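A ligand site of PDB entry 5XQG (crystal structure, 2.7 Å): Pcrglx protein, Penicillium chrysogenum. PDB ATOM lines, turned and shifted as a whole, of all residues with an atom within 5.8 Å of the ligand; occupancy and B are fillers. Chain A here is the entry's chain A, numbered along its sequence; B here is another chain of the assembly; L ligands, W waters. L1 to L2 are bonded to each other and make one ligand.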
ATOM      1  N   LEU A 430     -15.513  21.246  23.766  1.00  0.00           N
ATOM      2  CA  LEU A 430     -16.167  21.556  25.030  1.00  0.00           C
ATOM      3  C   LEU A 430     -15.219  22.149  26.057  1.00  0.00           C
ATOM      4  O   LEU A 430     -15.670  22.708  27.054  1.00  0.00           O
ATOM      5  CB  LEU A 430     -16.797  20.303  25.628  1.00  0.00           C
ATOM      6  CG  LEU A 430     -17.855  19.634  24.752  1.00  0.00           C
ATOM      7  CD1 LEU A 430     -18.104  18.191  25.230  1.00  0.00           C
ATOM      8  CD2 LEU A 430     -19.111  20.507  24.731  1.00  0.00           C
ATOM      9  N   LEU A 433     -15.464  25.747  25.045  1.00  0.00           N
ATOM     10  CA  LEU A 433     -16.745  26.152  25.647  1.00  0.00           C
ATOM     11  C   LEU A 433     -16.547  26.688  27.031  1.00  0.00           C
ATOM     12  O   LEU A 433     -17.106  27.719  27.345  1.00  0.00           O
ATOM     13  CB  LEU A 433     -17.789  25.027  25.643  1.00  0.00           C
ATOM     14  CG  LEU A 433     -19.208  25.379  26.096  1.00  0.00           C
ATOM     15  CD1 LEU A 433     -19.825  26.449  25.215  1.00  0.00           C
ATOM     16  CD2 LEU A 433     -20.138  24.165  26.127  1.00  0.00           C
ATOM     17  N   TYR A 437     -17.252  30.460  26.101  1.00  0.00           N
ATOM     18  CA  TYR A 437     -18.677  30.035  25.893  1.00  0.00           C
ATOM     19  C   TYR A 437     -19.047  29.750  24.416  1.00  0.00           C
ATOM     20  O   TYR A 437     -20.213  29.707  24.106  1.00  0.00           O
ATOM     21  CB  TYR A 437     -19.670  31.041  26.533  1.00  0.00           C
ATOM     22  CG  TYR A 437     -20.958  30.509  27.237  1.00  0.00           C
ATOM     23  CD1 TYR A 437     -20.962  29.322  27.992  1.00  0.00           C
ATOM     24  CD2 TYR A 437     -22.117  31.276  27.222  1.00  0.00           C
ATOM     25  CE1 TYR A 437     -22.114  28.898  28.673  1.00  0.00           C
ATOM     26  CE2 TYR A 437     -23.279  30.856  27.875  1.00  0.00           C
ATOM     27  CZ  TYR A 437     -23.296  29.679  28.615  1.00  0.00           C
ATOM     28  OH  TYR A 437     -24.477  29.279  29.278  1.00  0.00           O
ATOM     29  N   ASP A 439     -19.218  26.986  21.246  1.00  0.00           N
ATOM     30  CA  ASP A 439     -19.191  25.556  21.022  1.00  0.00           C
ATOM     31  C   ASP A 439     -18.900  25.357  19.546  1.00  0.00           C
ATOM     32  O   ASP A 439     -19.817  25.252  18.707  1.00  0.00           O
ATOM     33  CB  ASP A 439     -20.528  24.930  21.461  1.00  0.00           C
ATOM     34  CG  ASP A 439     -20.532  23.398  21.396  1.00  0.00           C
ATOM     35  OD1 ASP A 439     -19.419  22.839  21.307  1.00  0.00           O
ATOM     36  OD2 ASP A 439     -21.621  22.785  21.401  1.00  0.00           O
ATOM     37  N   GLU A 566     -31.366  34.136  22.713  1.00  0.00           N
ATOM     38  CA  GLU A 566     -31.083  33.280  23.873  1.00  0.00           C
ATOM     39  C   GLU A 566     -31.954  33.700  25.066  1.00  0.00           C
ATOM     40  O   GLU A 566     -32.008  34.898  25.416  1.00  0.00           O
ATOM     41  CB  GLU A 566     -29.608  33.368  24.240  1.00  0.00           C
ATOM     42  CG  GLU A 566     -29.165  32.521  25.432  1.00  0.00           C
ATOM     43  CD  GLU A 566     -29.215  31.007  25.214  1.00  0.00           C
ATOM     44  OE1 GLU A 566     -28.721  30.325  26.165  1.00  0.00           O
ATOM     45  OE2 GLU A 566     -29.697  30.503  24.142  1.00  0.00           O
ATOM     46  N   LEU A 567     -32.517  32.704  25.743  1.00  0.00           N
ATOM     47  CA  LEU A 567     -33.524  32.868  26.807  1.00  0.00           C
ATOM     48  C   LEU A 567     -34.744  33.719  26.427  1.00  0.00           C
ATOM     49  O   LEU A 567     -35.333  34.415  27.261  1.00  0.00           O
ATOM     50  CB  LEU A 567     -32.911  33.299  28.140  1.00  0.00           C
ATOM     51  CG  LEU A 567     -31.902  32.380  28.876  1.00  0.00           C
ATOM     52  CD1 LEU A 567     -32.046  32.543  30.406  1.00  0.00           C
ATOM     53  CD2 LEU A 567     -31.950  30.896  28.513  1.00  0.00           C
ATOM     54  N   ARG A 613     -27.035  29.133  17.800  1.00  0.00           N
ATOM     55  CA  ARG A 613     -26.821  29.667  19.143  1.00  0.00           C
ATOM     56  C   ARG A 613     -25.957  30.930  19.121  1.00  0.00           C
ATOM     57  O   ARG A 613     -25.061  31.092  18.266  1.00  0.00           O
ATOM     58  CB  ARG A 613     -26.175  28.607  20.019  1.00  0.00           C
ATOM     59  CG  ARG A 613     -25.734  29.005  21.414  1.00  0.00           C
ATOM     60  CD  ARG A 613     -25.185  27.755  22.090  1.00  0.00           C
ATOM     61  NE  ARG A 613     -24.594  27.988  23.396  1.00  0.00           N
ATOM     62  CZ  ARG A 613     -23.388  28.496  23.630  1.00  0.00           C
ATOM     63  NH1 ARG A 613     -22.608  28.866  22.620  1.00  0.00           N
ATOM     64  NH2 ARG A 613     -22.959  28.627  24.887  1.00  0.00           N
ATOM     65  N   HIS A 614     -26.272  31.840  20.044  1.00  0.00           N
ATOM     66  CA  HIS A 614     -25.495  33.064  20.314  1.00  0.00           C
ATOM     67  C   HIS A 614     -23.995  32.957  20.090  1.00  0.00           C
ATOM     68  O   HIS A 614     -23.321  32.117  20.689  1.00  0.00           O
ATOM     69  CB  HIS A 614     -25.746  33.591  21.739  1.00  0.00           C
ATOM     70  CG  HIS A 614     -25.732  32.566  22.810  1.00  0.00           C
ATOM     71  ND1 HIS A 614     -24.690  32.419  23.690  1.00  0.00           N
ATOM     72  CD2 HIS A 614     -26.662  31.669  23.192  1.00  0.00           C
ATOM     73  CE1 HIS A 614     -24.955  31.451  24.546  1.00  0.00           C
ATOM     74  NE2 HIS A 614     -26.143  30.968  24.259  1.00  0.00           N
ATOM     75  N   ASP A 621     -21.627  29.462  15.701  1.00  0.00           N
ATOM     76  CA  ASP A 621     -21.606  28.427  16.747  1.00  0.00           C
ATOM     77  C   ASP A 621     -22.153  27.115  16.197  1.00  0.00           C
ATOM     78  O   ASP A 621     -22.969  27.109  15.274  1.00  0.00           O
ATOM     79  CB  ASP A 621     -22.482  28.939  17.917  1.00  0.00           C
ATOM     80  CG  ASP A 621     -22.154  28.277  19.239  1.00  0.00           C
ATOM     81  OD1 ASP A 621     -21.276  28.779  20.001  1.00  0.00           O
ATOM     82  OD2 ASP A 621     -22.837  27.287  19.520  1.00  0.00           O
ATOM     83  N   SER A 622     -21.755  26.002  16.801  1.00  0.00           N
ATOM     84  CA  SER A 622     -22.152  24.681  16.318  1.00  0.00           C
ATOM     85  C   SER A 622     -23.435  24.163  16.884  1.00  0.00           C
ATOM     86  O   SER A 622     -23.928  23.189  16.369  1.00  0.00           O
ATOM     87  CB  SER A 622     -21.082  23.597  16.571  1.00  0.00           C
ATOM     88  OG  SER A 622     -21.209  22.987  17.861  1.00  0.00           O
ATOM     89  N   ALA A 623     -23.947  24.761  17.951  1.00  0.00           N
ATOM     90  CA  ALA A 623     -25.268  24.395  18.455  1.00  0.00           C
ATOM     91  C   ALA A 623     -26.310  24.881  17.468  1.00  0.00           C
ATOM     92  O   ALA A 623     -26.599  26.070  17.413  1.00  0.00           O
ATOM     93  CB  ALA A 623     -25.500  24.998  19.814  1.00  0.00           C
ATOM     94  N   GLN A 625     -30.067  24.474  16.613  1.00  0.00           N
ATOM     95  CA  GLN A 625     -31.149  24.058  17.436  1.00  0.00           C
ATOM     96  C   GLN A 625     -32.435  24.778  17.107  1.00  0.00           C
ATOM     97  O   GLN A 625     -32.454  25.977  16.727  1.00  0.00           O
ATOM     98  CB  GLN A 625     -30.789  24.243  18.911  1.00  0.00           C
ATOM     99  CG  GLN A 625     -29.816  23.211  19.416  1.00  0.00           C
ATOM    100  CD  GLN A 625     -29.686  23.251  20.920  1.00  0.00           C
ATOM    101  OE1 GLN A 625     -30.667  23.481  21.610  1.00  0.00           O
ATOM    102  NE2 GLN A 625     -28.453  23.074  21.439  1.00  0.00           N
ATOM    103  N   ARG A 627     -34.560  25.666  19.253  1.00  0.00           N
ATOM    104  CA  ARG A 627     -34.895  26.711  20.226  1.00  0.00           C
ATOM    105  C   ARG A 627     -34.557  28.112  19.717  1.00  0.00           C
ATOM    106  O   ARG A 627     -35.002  29.117  20.315  1.00  0.00           O
ATOM    107  CB  ARG A 627     -34.222  26.460  21.568  1.00  0.00           C
ATOM    108  CG  ARG A 627     -32.785  26.869  21.567  1.00  0.00           C
ATOM    109  CD  ARG A 627     -32.003  26.305  22.742  1.00  0.00           C
ATOM    110  NE  ARG A 627     -30.791  27.089  22.969  1.00  0.00           N
ATOM    111  CZ  ARG A 627     -29.684  26.632  23.512  1.00  0.00           C
ATOM    112  NH1 ARG A 627     -29.580  25.356  23.869  1.00  0.00           N
ATOM    113  NH2 ARG A 627     -28.663  27.464  23.692  1.00  0.00           N
ATOM    114  N   PRO A 666     -28.404  17.460  18.483  1.00  0.00           N
ATOM    115  CA  PRO A 666     -27.920  18.583  19.258  1.00  0.00           C
ATOM    116  C   PRO A 666     -27.171  18.153  20.513  1.00  0.00           C
ATOM    117  O   PRO A 666     -26.366  18.956  21.063  1.00  0.00           O
ATOM    118  CB  PRO A 666     -29.202  19.358  19.608  1.00  0.00           C
ATOM    119  CG  PRO A 666     -30.311  18.385  19.501  1.00  0.00           C
ATOM    120  CD  PRO A 666     -29.885  17.359  18.514  1.00  0.00           C
ATOM    121  N   GLN A 667     -27.455  16.911  20.963  1.00  0.00           N
ATOM    122  CA  GLN A 667     -26.784  16.317  22.138  1.00  0.00           C
ATOM    123  C   GLN A 667     -25.552  15.471  21.850  1.00  0.00           C
ATOM    124  O   GLN A 667     -24.956  14.908  22.788  1.00  0.00           O
ATOM    125  CB  GLN A 667     -27.810  15.562  22.986  1.00  0.00           C
ATOM    126  CG  GLN A 667     -28.984  16.436  23.490  1.00  0.00           C
ATOM    127  CD  GLN A 667     -28.554  17.505  24.492  1.00  0.00           C
ATOM    128  OE1 GLN A 667     -27.823  17.240  25.455  1.00  0.00           O
ATOM    129  NE2 GLN A 667     -28.996  18.727  24.256  1.00  0.00           N
ATOM    130  N   VAL A 670     -22.397  15.581  24.315  1.00  0.00           N
ATOM    131  CA  VAL A 670     -22.618  15.514  25.784  1.00  0.00           C
ATOM    132  C   VAL A 670     -23.429  14.297  26.249  1.00  0.00           C
ATOM    133  O   VAL A 670     -23.263  13.820  27.343  1.00  0.00           O
ATOM    134  CB  VAL A 670     -23.288  16.808  26.315  1.00  0.00           C
ATOM    135  CG1 VAL A 670     -22.409  18.006  26.002  1.00  0.00           C
ATOM    136  CG2 VAL A 670     -24.673  17.026  25.755  1.00  0.00           C
ATOM    137  N   HIS A 761     -31.831  23.165  33.137  1.00  0.00           N
ATOM    138  CA  HIS A 761     -32.269  24.516  33.416  1.00  0.00           C
ATOM    139  C   HIS A 761     -32.756  25.188  32.134  1.00  0.00           C
ATOM    140  O   HIS A 761     -33.600  26.064  32.183  1.00  0.00           O
ATOM    141  CB  HIS A 761     -31.197  25.323  34.178  1.00  0.00           C
ATOM    142  CG  HIS A 761     -29.971  25.654  33.373  1.00  0.00           C
ATOM    143  ND1 HIS A 761     -28.948  24.749  33.164  1.00  0.00           N
ATOM    144  CD2 HIS A 761     -29.593  26.795  32.745  1.00  0.00           C
ATOM    145  CE1 HIS A 761     -27.999  25.324  32.438  1.00  0.00           C
ATOM    146  NE2 HIS A 761     -28.374  26.560  32.160  1.00  0.00           N
ATOM    147  N   LEU A 762     -32.280  24.718  30.982  1.00  0.00           N
ATOM    148  CA  LEU A 762     -32.706  25.328  29.717  1.00  0.00           C
ATOM    149  C   LEU A 762     -34.109  24.942  29.232  1.00  0.00           C
ATOM    150  O   LEU A 762     -34.676  25.640  28.420  1.00  0.00           O
ATOM    151  CB  LEU A 762     -31.699  25.017  28.587  1.00  0.00           C
ATOM    152  CG  LEU A 762     -30.250  25.513  28.656  1.00  0.00           C
ATOM    153  CD1 LEU A 762     -29.594  25.063  27.355  1.00  0.00           C
ATOM    154  CD2 LEU A 762     -30.131  27.015  28.858  1.00  0.00           C
ATOM    155  N   PHE A 766     -37.245  28.573  26.680  1.00  0.00           N
ATOM    156  CA  PHE A 766     -37.304  28.877  25.260  1.00  0.00           C
ATOM    157  C   PHE A 766     -38.711  28.665  24.679  1.00  0.00           C
ATOM    158  O   PHE A 766     -38.849  28.320  23.500  1.00  0.00           O
ATOM    159  CB  PHE A 766     -36.301  28.013  24.518  1.00  0.00           C
ATOM    160  CG  PHE A 766     -34.876  28.271  24.896  1.00  0.00           C
ATOM    161  CD1 PHE A 766     -34.320  27.619  25.969  1.00  0.00           C
ATOM    162  CD2 PHE A 766     -34.105  29.161  24.176  1.00  0.00           C
ATOM    163  CE1 PHE A 766     -32.984  27.846  26.320  1.00  0.00           C
ATOM    164  CE2 PHE A 766     -32.773  29.403  24.520  1.00  0.00           C
ATOM    165  CZ  PHE A 766     -32.198  28.764  25.585  1.00  0.00           C
ATOM    166  N   ASN A 881     -29.667  37.488  29.307  1.00  0.00           N
ATOM    167  CA  ASN A 881     -30.315  36.327  29.887  1.00  0.00           C
ATOM    168  C   ASN A 881     -31.177  36.701  31.077  1.00  0.00           C
ATOM    169  O   ASN A 881     -32.308  36.193  31.216  1.00  0.00           O
ATOM    170  CB  ASN A 881     -29.288  35.255  30.257  1.00  0.00           C
ATOM    171  CG  ASN A 881     -28.855  34.439  29.061  1.00  0.00           C
ATOM    172  OD1 ASN A 881     -29.276  34.684  27.930  1.00  0.00           O
ATOM    173  ND2 ASN A 881     -28.047  33.480  29.311  1.00  0.00           N
ATOM    174  N   ARG B 288     -15.618  33.581  30.171  1.00  0.00           N
ATOM    175  CA  ARG B 288     -16.508  32.830  31.023  1.00  0.00           C
ATOM    176  C   ARG B 288     -15.929  32.650  32.406  1.00  0.00           C
ATOM    177  O   ARG B 288     -16.662  32.681  33.353  1.00  0.00           O
ATOM    178  CB  ARG B 288     -16.758  31.487  30.439  1.00  0.00           C
ATOM    179  CG  ARG B 288     -17.754  30.697  31.239  1.00  0.00           C
ATOM    180  CD  ARG B 288     -18.339  29.561  30.427  1.00  0.00           C
ATOM    181  NE  ARG B 288     -19.286  28.833  31.270  1.00  0.00           N
ATOM    182  CZ  ARG B 288     -19.751  27.615  31.042  1.00  0.00           C
ATOM    183  NH1 ARG B 288     -19.409  26.908  29.942  1.00  0.00           N
ATOM    184  NH2 ARG B 288     -20.589  27.091  31.926  1.00  0.00           N
HETATM  185  C1  LIG L   1     -23.733  23.651  24.109  1.00  0.00           C
HETATM  186  C2  LIG L   1     -24.740  24.628  24.678  1.00  0.00           C
HETATM  187  C3  LIG L   1     -26.175  24.279  24.303  1.00  0.00           C
HETATM  188  C4  LIG L   1     -26.522  22.849  24.671  1.00  0.00           C
HETATM  189  C5  LIG L   1     -25.405  21.905  24.165  1.00  0.00           C
HETATM  190  C6  LIG L   1     -25.560  20.508  24.728  1.00  0.00           C
HETATM  191  O1  LIG L   1     -23.775  23.855  22.703  1.00  0.00           O
HETATM  192  O2  LIG L   1     -24.573  24.632  26.113  1.00  0.00           O
HETATM  193  O3  LIG L   1     -27.085  25.170  24.948  1.00  0.00           O
HETATM  194  O4  LIG L   1     -27.834  22.651  24.173  1.00  0.00           O
HETATM  195  O5  LIG L   1     -24.083  22.331  24.550  1.00  0.00           O
HETATM  196  C1  LG2 L   2     -23.738  25.505  26.760  1.00  0.00           C
HETATM  197  C2  LG2 L   2     -23.730  25.279  28.261  1.00  0.00           C
HETATM  198  O1  LG2 L   2     -23.089  24.058  28.509  1.00  0.00           O
HETATM  199  C3  LG2 L   2     -25.139  25.214  28.814  1.00  0.00           C
HETATM  200  O2  LG2 L   2     -25.014  25.200  30.229  1.00  0.00           O
HETATM  201  C4  LG2 L   2     -25.953  26.415  28.362  1.00  0.00           C
HETATM  202  C5  LG2 L   2     -25.675  27.036  27.210  1.00  0.00           C
HETATM  203  C6  LG2 L   2     -26.504  28.050  26.641  1.00  0.00           C
HETATM  204  O3  LG2 L   2     -27.585  28.391  27.141  1.00  0.00           O
HETATM  205  O4  LG2 L   2     -26.088  28.566  25.592  1.00  0.00           O
HETATM  206  O5  LG2 L   2     -24.523  26.671  26.432  1.00  0.00           O
HETATM  207  O   HOH W   1     -22.398  20.630  22.593  1.00  0.00           O
HETATM  208  O   HOH W   2     -26.514  31.252  27.880  1.00  0.00           O
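O of Tyr 437 is in hydrogen-bond range of NH1 of Arg 613 (2.9 Å).
The guanidinium group of Arg 613 lies within salt-bridge range of the side-chain carboxylate of Asp 621.
The guanidinium group of Arg 627 sits at hydrogen-bond distance from the side-chain amide oxygen of Gln 625 (3.1 Å).
OE1 of Glu 566 sits close to NE2 of His 614 (3.3 Å).
The guanidinium group (NH2) of Arg 627 is in salt-bridge range of the side-chain carboxylate (OE2) of Glu 566.
The backbone NH (N) of Asp 439 is in hydrogen-bond range of the side-chain carboxylate (OD1) of Asp 621, at 3.0 Å.
The backbone carbonyl oxygen (O) of Asp 439 sits at hydrogen-bond distance from the side-chain hydroxyl (OG) of Ser 622 (2.8 Å).
N of Ala 623 is in hydrogen-bond range of OD2 of Asp 621, at 3.2 Å.
An oxygen (O4) of LG2 L2 is in salt-bridge range of the guanidinium group (NH2) of Arg 627.
OE1 of Glu 566 sits close to O3 of LG2 L2 (2.4 Å).
The side-chain amide nitrogen of Gln 625 sits at hydrogen-bond distance from an oxygen (O4) of LIG L1 (2.8 Å).
NE of Arg 613 lies within salt-bridge range of O4 of LG2 L2, 2.7 Å away.
NE2 of His 614 lies within hydrogen-bond range of O4 of LG2 L2, 2.7 Å away.
The side-chain carboxylate (OD2) of Asp 439 lies within hydrogen-bond range of an oxygen (O1) of LIG L1.
Water W1 lies within hydrogen-bond range of OD2 of Asp 439 (2.6 Å) and O5 of LIG L1 (3.1 Å).
Water W2 lies within hydrogen-bond range of OE1 of Glu 566, ND2 of Asn 881, O3 of LG2 L2 and OH of Tyr 437.
Residues that only touch the ligand: Leu 433, Tyr 437, Ala 623, Gln 667, Val 670, His 761 and Leu 762.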
